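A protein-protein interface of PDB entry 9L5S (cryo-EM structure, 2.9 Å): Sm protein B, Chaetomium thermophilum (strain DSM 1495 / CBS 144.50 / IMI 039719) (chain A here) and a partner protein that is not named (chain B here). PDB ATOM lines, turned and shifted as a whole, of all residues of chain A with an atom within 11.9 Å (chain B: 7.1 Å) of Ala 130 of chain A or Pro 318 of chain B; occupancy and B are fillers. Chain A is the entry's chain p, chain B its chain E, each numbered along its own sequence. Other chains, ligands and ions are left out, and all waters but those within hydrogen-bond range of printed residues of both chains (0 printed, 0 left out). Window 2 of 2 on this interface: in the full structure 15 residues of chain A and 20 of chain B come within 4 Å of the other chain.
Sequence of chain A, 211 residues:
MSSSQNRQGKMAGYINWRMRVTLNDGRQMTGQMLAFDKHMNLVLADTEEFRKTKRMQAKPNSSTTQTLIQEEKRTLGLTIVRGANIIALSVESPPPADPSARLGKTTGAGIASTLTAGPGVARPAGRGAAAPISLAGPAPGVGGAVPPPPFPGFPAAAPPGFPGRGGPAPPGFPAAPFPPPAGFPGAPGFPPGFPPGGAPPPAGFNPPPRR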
ATOM      1  N   ARG A 123      25.832   6.541 -13.397  1.00  0.00           N
ATOM      2  CA  ARG A 123      27.159   6.064 -13.046  1.00  0.00           C
ATOM      3  C   ARG A 123      27.547   4.932 -13.984  1.00  0.00           C
ATOM      4  O   ARG A 123      26.672   4.243 -14.523  1.00  0.00           O
ATOM      5  CB  ARG A 123      27.215   5.586 -11.585  1.00  0.00           C
ATOM      6  CG  ARG A 123      26.354   4.372 -11.278  1.00  0.00           C
ATOM      7  CD  ARG A 123      26.816   3.663 -10.014  1.00  0.00           C
ATOM      8  NE  ARG A 123      26.038   2.460  -9.743  1.00  0.00           N
ATOM      9  CZ  ARG A 123      26.266   1.276 -10.296  1.00  0.00           C
ATOM     10  NH1 ARG A 123      27.264   1.091 -11.144  1.00  0.00           N
ATOM     11  NH2 ARG A 123      25.477   0.252  -9.986  1.00  0.00           N
ATOM     12  N   ALA A 125      28.773   1.240 -15.135  1.00  0.00           N
ATOM     13  CA  ALA A 125      28.421  -0.072 -14.610  1.00  0.00           C
ATOM     14  C   ALA A 125      28.834  -1.130 -15.621  1.00  0.00           C
ATOM     15  O   ALA A 125      29.149  -0.831 -16.774  1.00  0.00           O
ATOM     16  CB  ALA A 125      26.926  -0.168 -14.300  1.00  0.00           C
ATOM     17  N   GLY A 126      28.832  -2.378 -15.167  1.00  0.00           N
ATOM     18  CA  GLY A 126      29.106  -3.497 -16.043  1.00  0.00           C
ATOM     19  C   GLY A 126      27.923  -4.436 -16.125  1.00  0.00           C
ATOM     20  O   GLY A 126      27.004  -4.351 -15.307  1.00  0.00           O
ATOM     21  N   ARG A 127      27.927  -5.337 -17.106  1.00  0.00           N
ATOM     22  CA  ARG A 127      26.843  -6.302 -17.248  1.00  0.00           C
ATOM     23  C   ARG A 127      26.967  -7.486 -16.297  1.00  0.00           C
ATOM     24  O   ARG A 127      26.204  -8.447 -16.433  1.00  0.00           O
ATOM     25  CB  ARG A 127      26.775  -6.813 -18.688  1.00  0.00           C
ATOM     26  CG  ARG A 127      26.239  -5.794 -19.663  1.00  0.00           C
ATOM     27  CD  ARG A 127      25.633  -6.435 -20.896  1.00  0.00           C
ATOM     28  NE  ARG A 127      25.185  -5.422 -21.843  1.00  0.00           N
ATOM     29  CZ  ARG A 127      23.970  -4.893 -21.853  1.00  0.00           C
ATOM     30  NH1 ARG A 127      23.042  -5.275 -20.991  1.00  0.00           N
ATOM     31  NH2 ARG A 127      23.679  -3.953 -22.748  1.00  0.00           N
ATOM     32  N   GLY A 128      27.896  -7.444 -15.348  1.00  0.00           N
ATOM     33  CA  GLY A 128      28.068  -8.533 -14.413  1.00  0.00           C
ATOM     34  C   GLY A 128      28.735  -9.730 -15.055  1.00  0.00           C
ATOM     35  O   GLY A 128      29.212  -9.698 -16.190  1.00  0.00           O
ATOM     36  N   ALA A 129      28.765 -10.820 -14.294  1.00  0.00           N
ATOM     37  CA  ALA A 129      29.322 -12.083 -14.767  1.00  0.00           C
ATOM     38  C   ALA A 129      28.192 -12.889 -15.391  1.00  0.00           C
ATOM     39  O   ALA A 129      27.320 -13.404 -14.689  1.00  0.00           O
ATOM     40  CB  ALA A 129      29.990 -12.840 -13.625  1.00  0.00           C
ATOM     41  N   ALA A 130      28.198 -12.977 -16.721  1.00  0.00           N
ATOM     42  CA  ALA A 130      27.219 -13.789 -17.429  1.00  0.00           C
ATOM     43  C   ALA A 130      27.395 -15.261 -17.081  1.00  0.00           C
ATOM     44  O   ALA A 130      28.516 -15.736 -16.877  1.00  0.00           O
ATOM     45  CB  ALA A 130      27.353 -13.591 -18.938  1.00  0.00           C
ATOM     46  N   ALA A 131      26.282 -15.977 -17.002  1.00  0.00           N
ATOM     47  CA  ALA A 131      26.332 -17.407 -16.727  1.00  0.00           C
ATOM     48  C   ALA A 131      26.920 -18.129 -17.931  1.00  0.00           C
ATOM     49  O   ALA A 131      26.353 -18.045 -19.029  1.00  0.00           O
ATOM     50  CB  ALA A 131      24.939 -17.941 -16.410  1.00  0.00           C
ATOM     51  N   PRO A 132      28.042 -18.835 -17.783  1.00  0.00           N
ATOM     52  CA  PRO A 132      28.666 -19.477 -18.948  1.00  0.00           C
ATOM     53  C   PRO A 132      27.895 -20.700 -19.420  1.00  0.00           C
ATOM     54  O   PRO A 132      27.943 -21.764 -18.797  1.00  0.00           O
ATOM     55  CB  PRO A 132      30.066 -19.845 -18.437  1.00  0.00           C
ATOM     56  CG  PRO A 132      29.927 -19.944 -16.958  1.00  0.00           C
ATOM     57  CD  PRO A 132      28.831 -19.004 -16.551  1.00  0.00           C
ATOM     58  N   ILE A 133      27.183 -20.549 -20.532  1.00  0.00           N
ATOM     59  CA  ILE A 133      26.361 -21.624 -21.072  1.00  0.00           C
ATOM     60  C   ILE A 133      27.142 -22.421 -22.109  1.00  0.00           C
ATOM     61  O   ILE A 133      28.322 -22.721 -21.918  1.00  0.00           O
ATOM     62  CB  ILE A 133      25.057 -21.070 -21.674  1.00  0.00           C
ATOM     63  CG1 ILE A 133      24.253 -20.324 -20.607  1.00  0.00           C
ATOM     64  CG2 ILE A 133      24.234 -22.192 -22.289  1.00  0.00           C
ATOM     65  CD1 ILE A 133      22.971 -19.707 -21.123  1.00  0.00           C
ATOM     66  N   LEU B  53      29.363   1.185 -20.966  1.00  0.00           N
ATOM     67  CA  LEU B  53      28.029   0.847 -20.499  1.00  0.00           C
ATOM     68  C   LEU B  53      27.834   1.487 -19.136  1.00  0.00           C
ATOM     69  O   LEU B  53      28.767   1.538 -18.331  1.00  0.00           O
ATOM     70  CB  LEU B  53      27.824  -0.668 -20.436  1.00  0.00           C
ATOM     71  CG  LEU B  53      26.419  -1.177 -20.131  1.00  0.00           C
ATOM     72  CD1 LEU B  53      26.212  -2.397 -20.956  1.00  0.00           C
ATOM     73  CD2 LEU B  53      26.267  -1.539 -18.663  1.00  0.00           C
ATOM     74  N   ASP B 300      15.018 -13.030 -17.771  1.00  0.00           N
ATOM     75  CA  ASP B 300      16.212 -13.367 -17.009  1.00  0.00           C
ATOM     76  C   ASP B 300      17.077 -12.152 -16.713  1.00  0.00           C
ATOM     77  O   ASP B 300      18.182 -12.306 -16.183  1.00  0.00           O
ATOM     78  CB  ASP B 300      17.042 -14.410 -17.762  1.00  0.00           C
ATOM     79  CG  ASP B 300      16.270 -15.681 -18.042  1.00  0.00           C
ATOM     80  OD1 ASP B 300      15.176 -15.856 -17.467  1.00  0.00           O
ATOM     81  OD2 ASP B 300      16.760 -16.508 -18.839  1.00  0.00           O
ATOM     82  N   GLY B 301      16.606 -10.953 -17.044  1.00  0.00           N
ATOM     83  CA  GLY B 301      17.437  -9.775 -16.955  1.00  0.00           C
ATOM     84  C   GLY B 301      18.345  -9.562 -18.140  1.00  0.00           C
ATOM     85  O   GLY B 301      19.183  -8.654 -18.105  1.00  0.00           O
ATOM     86  N   THR B 302      18.207 -10.369 -19.187  1.00  0.00           N
ATOM     87  CA  THR B 302      19.051 -10.294 -20.365  1.00  0.00           C
ATOM     88  C   THR B 302      18.290  -9.671 -21.528  1.00  0.00           C
ATOM     89  O   THR B 302      17.058  -9.702 -21.588  1.00  0.00           O
ATOM     90  CB  THR B 302      19.554 -11.683 -20.772  1.00  0.00           C
ATOM     91  OG1 THR B 302      18.437 -12.525 -21.079  1.00  0.00           O
ATOM     92  CG2 THR B 302      20.353 -12.312 -19.645  1.00  0.00           C
ATOM     93  N   VAL B 303      19.050  -9.088 -22.447  1.00  0.00           N
ATOM     94  CA  VAL B 303      18.545  -8.618 -23.730  1.00  0.00           C
ATOM     95  C   VAL B 303      19.088  -9.555 -24.793  1.00  0.00           C
ATOM     96  O   VAL B 303      20.308  -9.699 -24.932  1.00  0.00           O
ATOM     97  CB  VAL B 303      18.966  -7.170 -24.012  1.00  0.00           C
ATOM     98  CG1 VAL B 303      18.384  -6.713 -25.329  1.00  0.00           C
ATOM     99  CG2 VAL B 303      18.530  -6.262 -22.881  1.00  0.00           C
ATOM    100  N   LYS B 316      23.377 -12.138 -25.891  1.00  0.00           N
ATOM    101  CA  LYS B 316      22.521 -12.341 -24.717  1.00  0.00           C
ATOM    102  C   LYS B 316      23.157 -11.532 -23.590  1.00  0.00           C
ATOM    103  O   LYS B 316      24.094 -11.990 -22.931  1.00  0.00           O
ATOM    104  CB  LYS B 316      22.366 -13.809 -24.349  1.00  0.00           C
ATOM    105  CG  LYS B 316      21.240 -14.039 -23.356  1.00  0.00           C
ATOM    106  CD  LYS B 316      21.077 -15.499 -22.983  1.00  0.00           C
ATOM    107  CE  LYS B 316      20.099 -15.646 -21.826  1.00  0.00           C
ATOM    108  NZ  LYS B 316      20.070 -17.026 -21.270  1.00  0.00           N
ATOM    109  N   LEU B 317      22.633 -10.326 -23.373  1.00  0.00           N
ATOM    110  CA  LEU B 317      23.282  -9.337 -22.528  1.00  0.00           C
ATOM    111  C   LEU B 317      22.681  -9.353 -21.128  1.00  0.00           C
ATOM    112  O   LEU B 317      21.515  -8.965 -20.964  1.00  0.00           O
ATOM    113  CB  LEU B 317      23.137  -7.957 -23.146  1.00  0.00           C
ATOM    114  CG  LEU B 317      23.644  -7.799 -24.579  1.00  0.00           C
ATOM    115  CD1 LEU B 317      23.181  -6.479 -25.166  1.00  0.00           C
ATOM    116  CD2 LEU B 317      25.156  -7.897 -24.617  1.00  0.00           C
ATOM    117  N   PRO B 318      23.423  -9.759 -20.101  1.00  0.00           N
ATOM    118  CA  PRO B 318      22.889  -9.717 -18.734  1.00  0.00           C
ATOM    119  C   PRO B 318      23.043  -8.347 -18.094  1.00  0.00           C
ATOM    120  O   PRO B 318      23.411  -7.379 -18.765  1.00  0.00           O
ATOM    121  CB  PRO B 318      23.725 -10.773 -18.008  1.00  0.00           C
ATOM    122  CG  PRO B 318      25.042 -10.717 -18.703  1.00  0.00           C
ATOM    123  CD  PRO B 318      24.780 -10.331 -20.142  1.00  0.00           C
ATOM    124  N   GLY B 319      22.745  -8.245 -16.803  1.00  0.00           N
ATOM    125  CA  GLY B 319      22.954  -7.012 -16.063  1.00  0.00           C
ATOM    126  C   GLY B 319      21.727  -6.470 -15.364  1.00  0.00           C
ATOM    127  O   GLY B 319      21.824  -5.423 -14.710  1.00  0.00           O
ATOM    128  N   HIS B 320      20.576  -7.124 -15.469  1.00  0.00           N
ATOM    129  CA  HIS B 320      19.356  -6.675 -14.819  1.00  0.00           C
ATOM    130  C   HIS B 320      18.871  -7.747 -13.855  1.00  0.00           C
ATOM    131  O   HIS B 320      19.067  -8.944 -14.083  1.00  0.00           O
ATOM    132  CB  HIS B 320      18.264  -6.364 -15.848  1.00  0.00           C
ATOM    133  CG  HIS B 320      18.535  -5.139 -16.664  1.00  0.00           C
ATOM    134  ND1 HIS B 320      18.466  -3.866 -16.142  1.00  0.00           N
ATOM    135  CD2 HIS B 320      18.875  -4.993 -17.967  1.00  0.00           C
ATOM    136  CE1 HIS B 320      18.750  -2.988 -17.087  1.00  0.00           C
ATOM    137  NE2 HIS B 320      19.003  -3.647 -18.204  1.00  0.00           N
ATOM    138  N   SER B 339      18.352  -0.619 -22.408  1.00  0.00           N
ATOM    139  CA  SER B 339      17.461  -1.591 -21.794  1.00  0.00           C
ATOM    140  C   SER B 339      16.810  -0.973 -20.568  1.00  0.00           C
ATOM    141  O   SER B 339      17.482  -0.346 -19.750  1.00  0.00           O
ATOM    142  CB  SER B 339      18.212  -2.865 -21.405  1.00  0.00           C
ATOM    143  OG  SER B 339      19.173  -2.599 -20.400  1.00  0.00           O
ATOM    144  N   LEU B 347      19.993   0.383 -18.592  1.00  0.00           N
ATOM    145  CA  LEU B 347      21.387   0.240 -18.992  1.00  0.00           C
ATOM    146  C   LEU B 347      21.560   0.831 -20.384  1.00  0.00           C
ATOM    147  O   LEU B 347      20.837   0.455 -21.313  1.00  0.00           O
ATOM    148  CB  LEU B 347      21.825  -1.226 -18.988  1.00  0.00           C
ATOM    149  CG  LEU B 347      22.029  -1.930 -17.647  1.00  0.00           C
ATOM    150  CD1 LEU B 347      22.452  -3.374 -17.864  1.00  0.00           C
ATOM    151  CD2 LEU B 347      23.052  -1.197 -16.817  1.00  0.00           C
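The backbone NH (N) of Ala 125 of chain A lies within hydrogen-bond range of the backbone carbonyl oxygen (O) of Leu 53 of chain B (3.2 Å). NH1 of Arg 127 of chain A sits at hydrogen-bond distance from O of Pro 318 of chain B, 3.1 Å away. The backbone carbonyl oxygen (O) of Arg 127 of chain A is in hydrogen-bond range of the backbone NH (N) of Gly 319 of chain B, 3.5 Å away.
The backbone carbonyl oxygen of Val 303 of chain B lies within hydrogen-bond range of the backbone NH of Leu 317 of chain B, at 2.9 Å. O of Ser 339 of chain B is in hydrogen-bond range of N of Leu 347 of chain B (2.9 Å).
Arg 127 of chain A touches Leu 53 of chain B (NE to CD1, 3.3 Å). Arg 127 of chain A touches Leu 317 of chain B (CZ to CB, 3.4 Å). CD1 of Leu 347 of chain B touches NH1 of Arg 127 of chain A (3.7 Å). CG of Pro 318 of chain B touches CB of Ala 130 of chain A, 3.7 Å away. Ile 133 of chain A touches Lys 316 of chain B.
Of chain B, only Pro 318 comes within 4 Å of Ala 130 of chain A. Pro 318 of chain B touches just these residues of chain A: Arg 127 (3.1 Å) and Ala 130 (3.7 Å). No residue of chain A comes within 4 Å of Gly 301 of chain B. No residue of chain A comes within 4 Å of Thr 302 of chain B. Of the printed residues of chain A, Leu 317 of chain B touches Arg 127 (3.4 Å). Of the printed residues of chain B, Ala 125 of chain A touches Leu 53. Of the printed residues of chain A, Leu 347 of chain B touches Arg 127. Of the printed residues of chain B, Ile 133 of chain A touches Lys 316 (3.95 Å). Printed residues of chain B within 4 Å of Arg 127 of chain A: Leu 53, Leu 317, Pro 318, Gly 319 and Leu 347. Ser 339 of chain B touches none of the printed residues of chain A. Ala 129 of chain A touches none of the printed residues of chain B. The nearest residue of chain B that does not touch Ala 130 of chain A is Lys 316 of chain B (5.4 Å). The nearest printed residue of chain B that does not touch Ala 125 of chain A is Leu 347 of chain B (4.7 Å).
Hydrophobic or aromatic side chains of chain B within 4 Å of the printed part of chain A: Leu 53, Leu 317, Pro 318 and Leu 347. Of the 10 printed residues of chain A, 4 touch a printed residue of chain B. Printed residues of chain A that touch a printed residue of chain B: Ala 125, Arg 127, Ala 130 and Ile 133. Hydrophobic or aromatic side chains of chain A that line the printed part of chain B: Ala 130 and Ile 133. Among the printed residues, no Asp or Glu carboxylate lies within 4 Å of a Lys or Arg side-chain nitrogen of the other chain.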
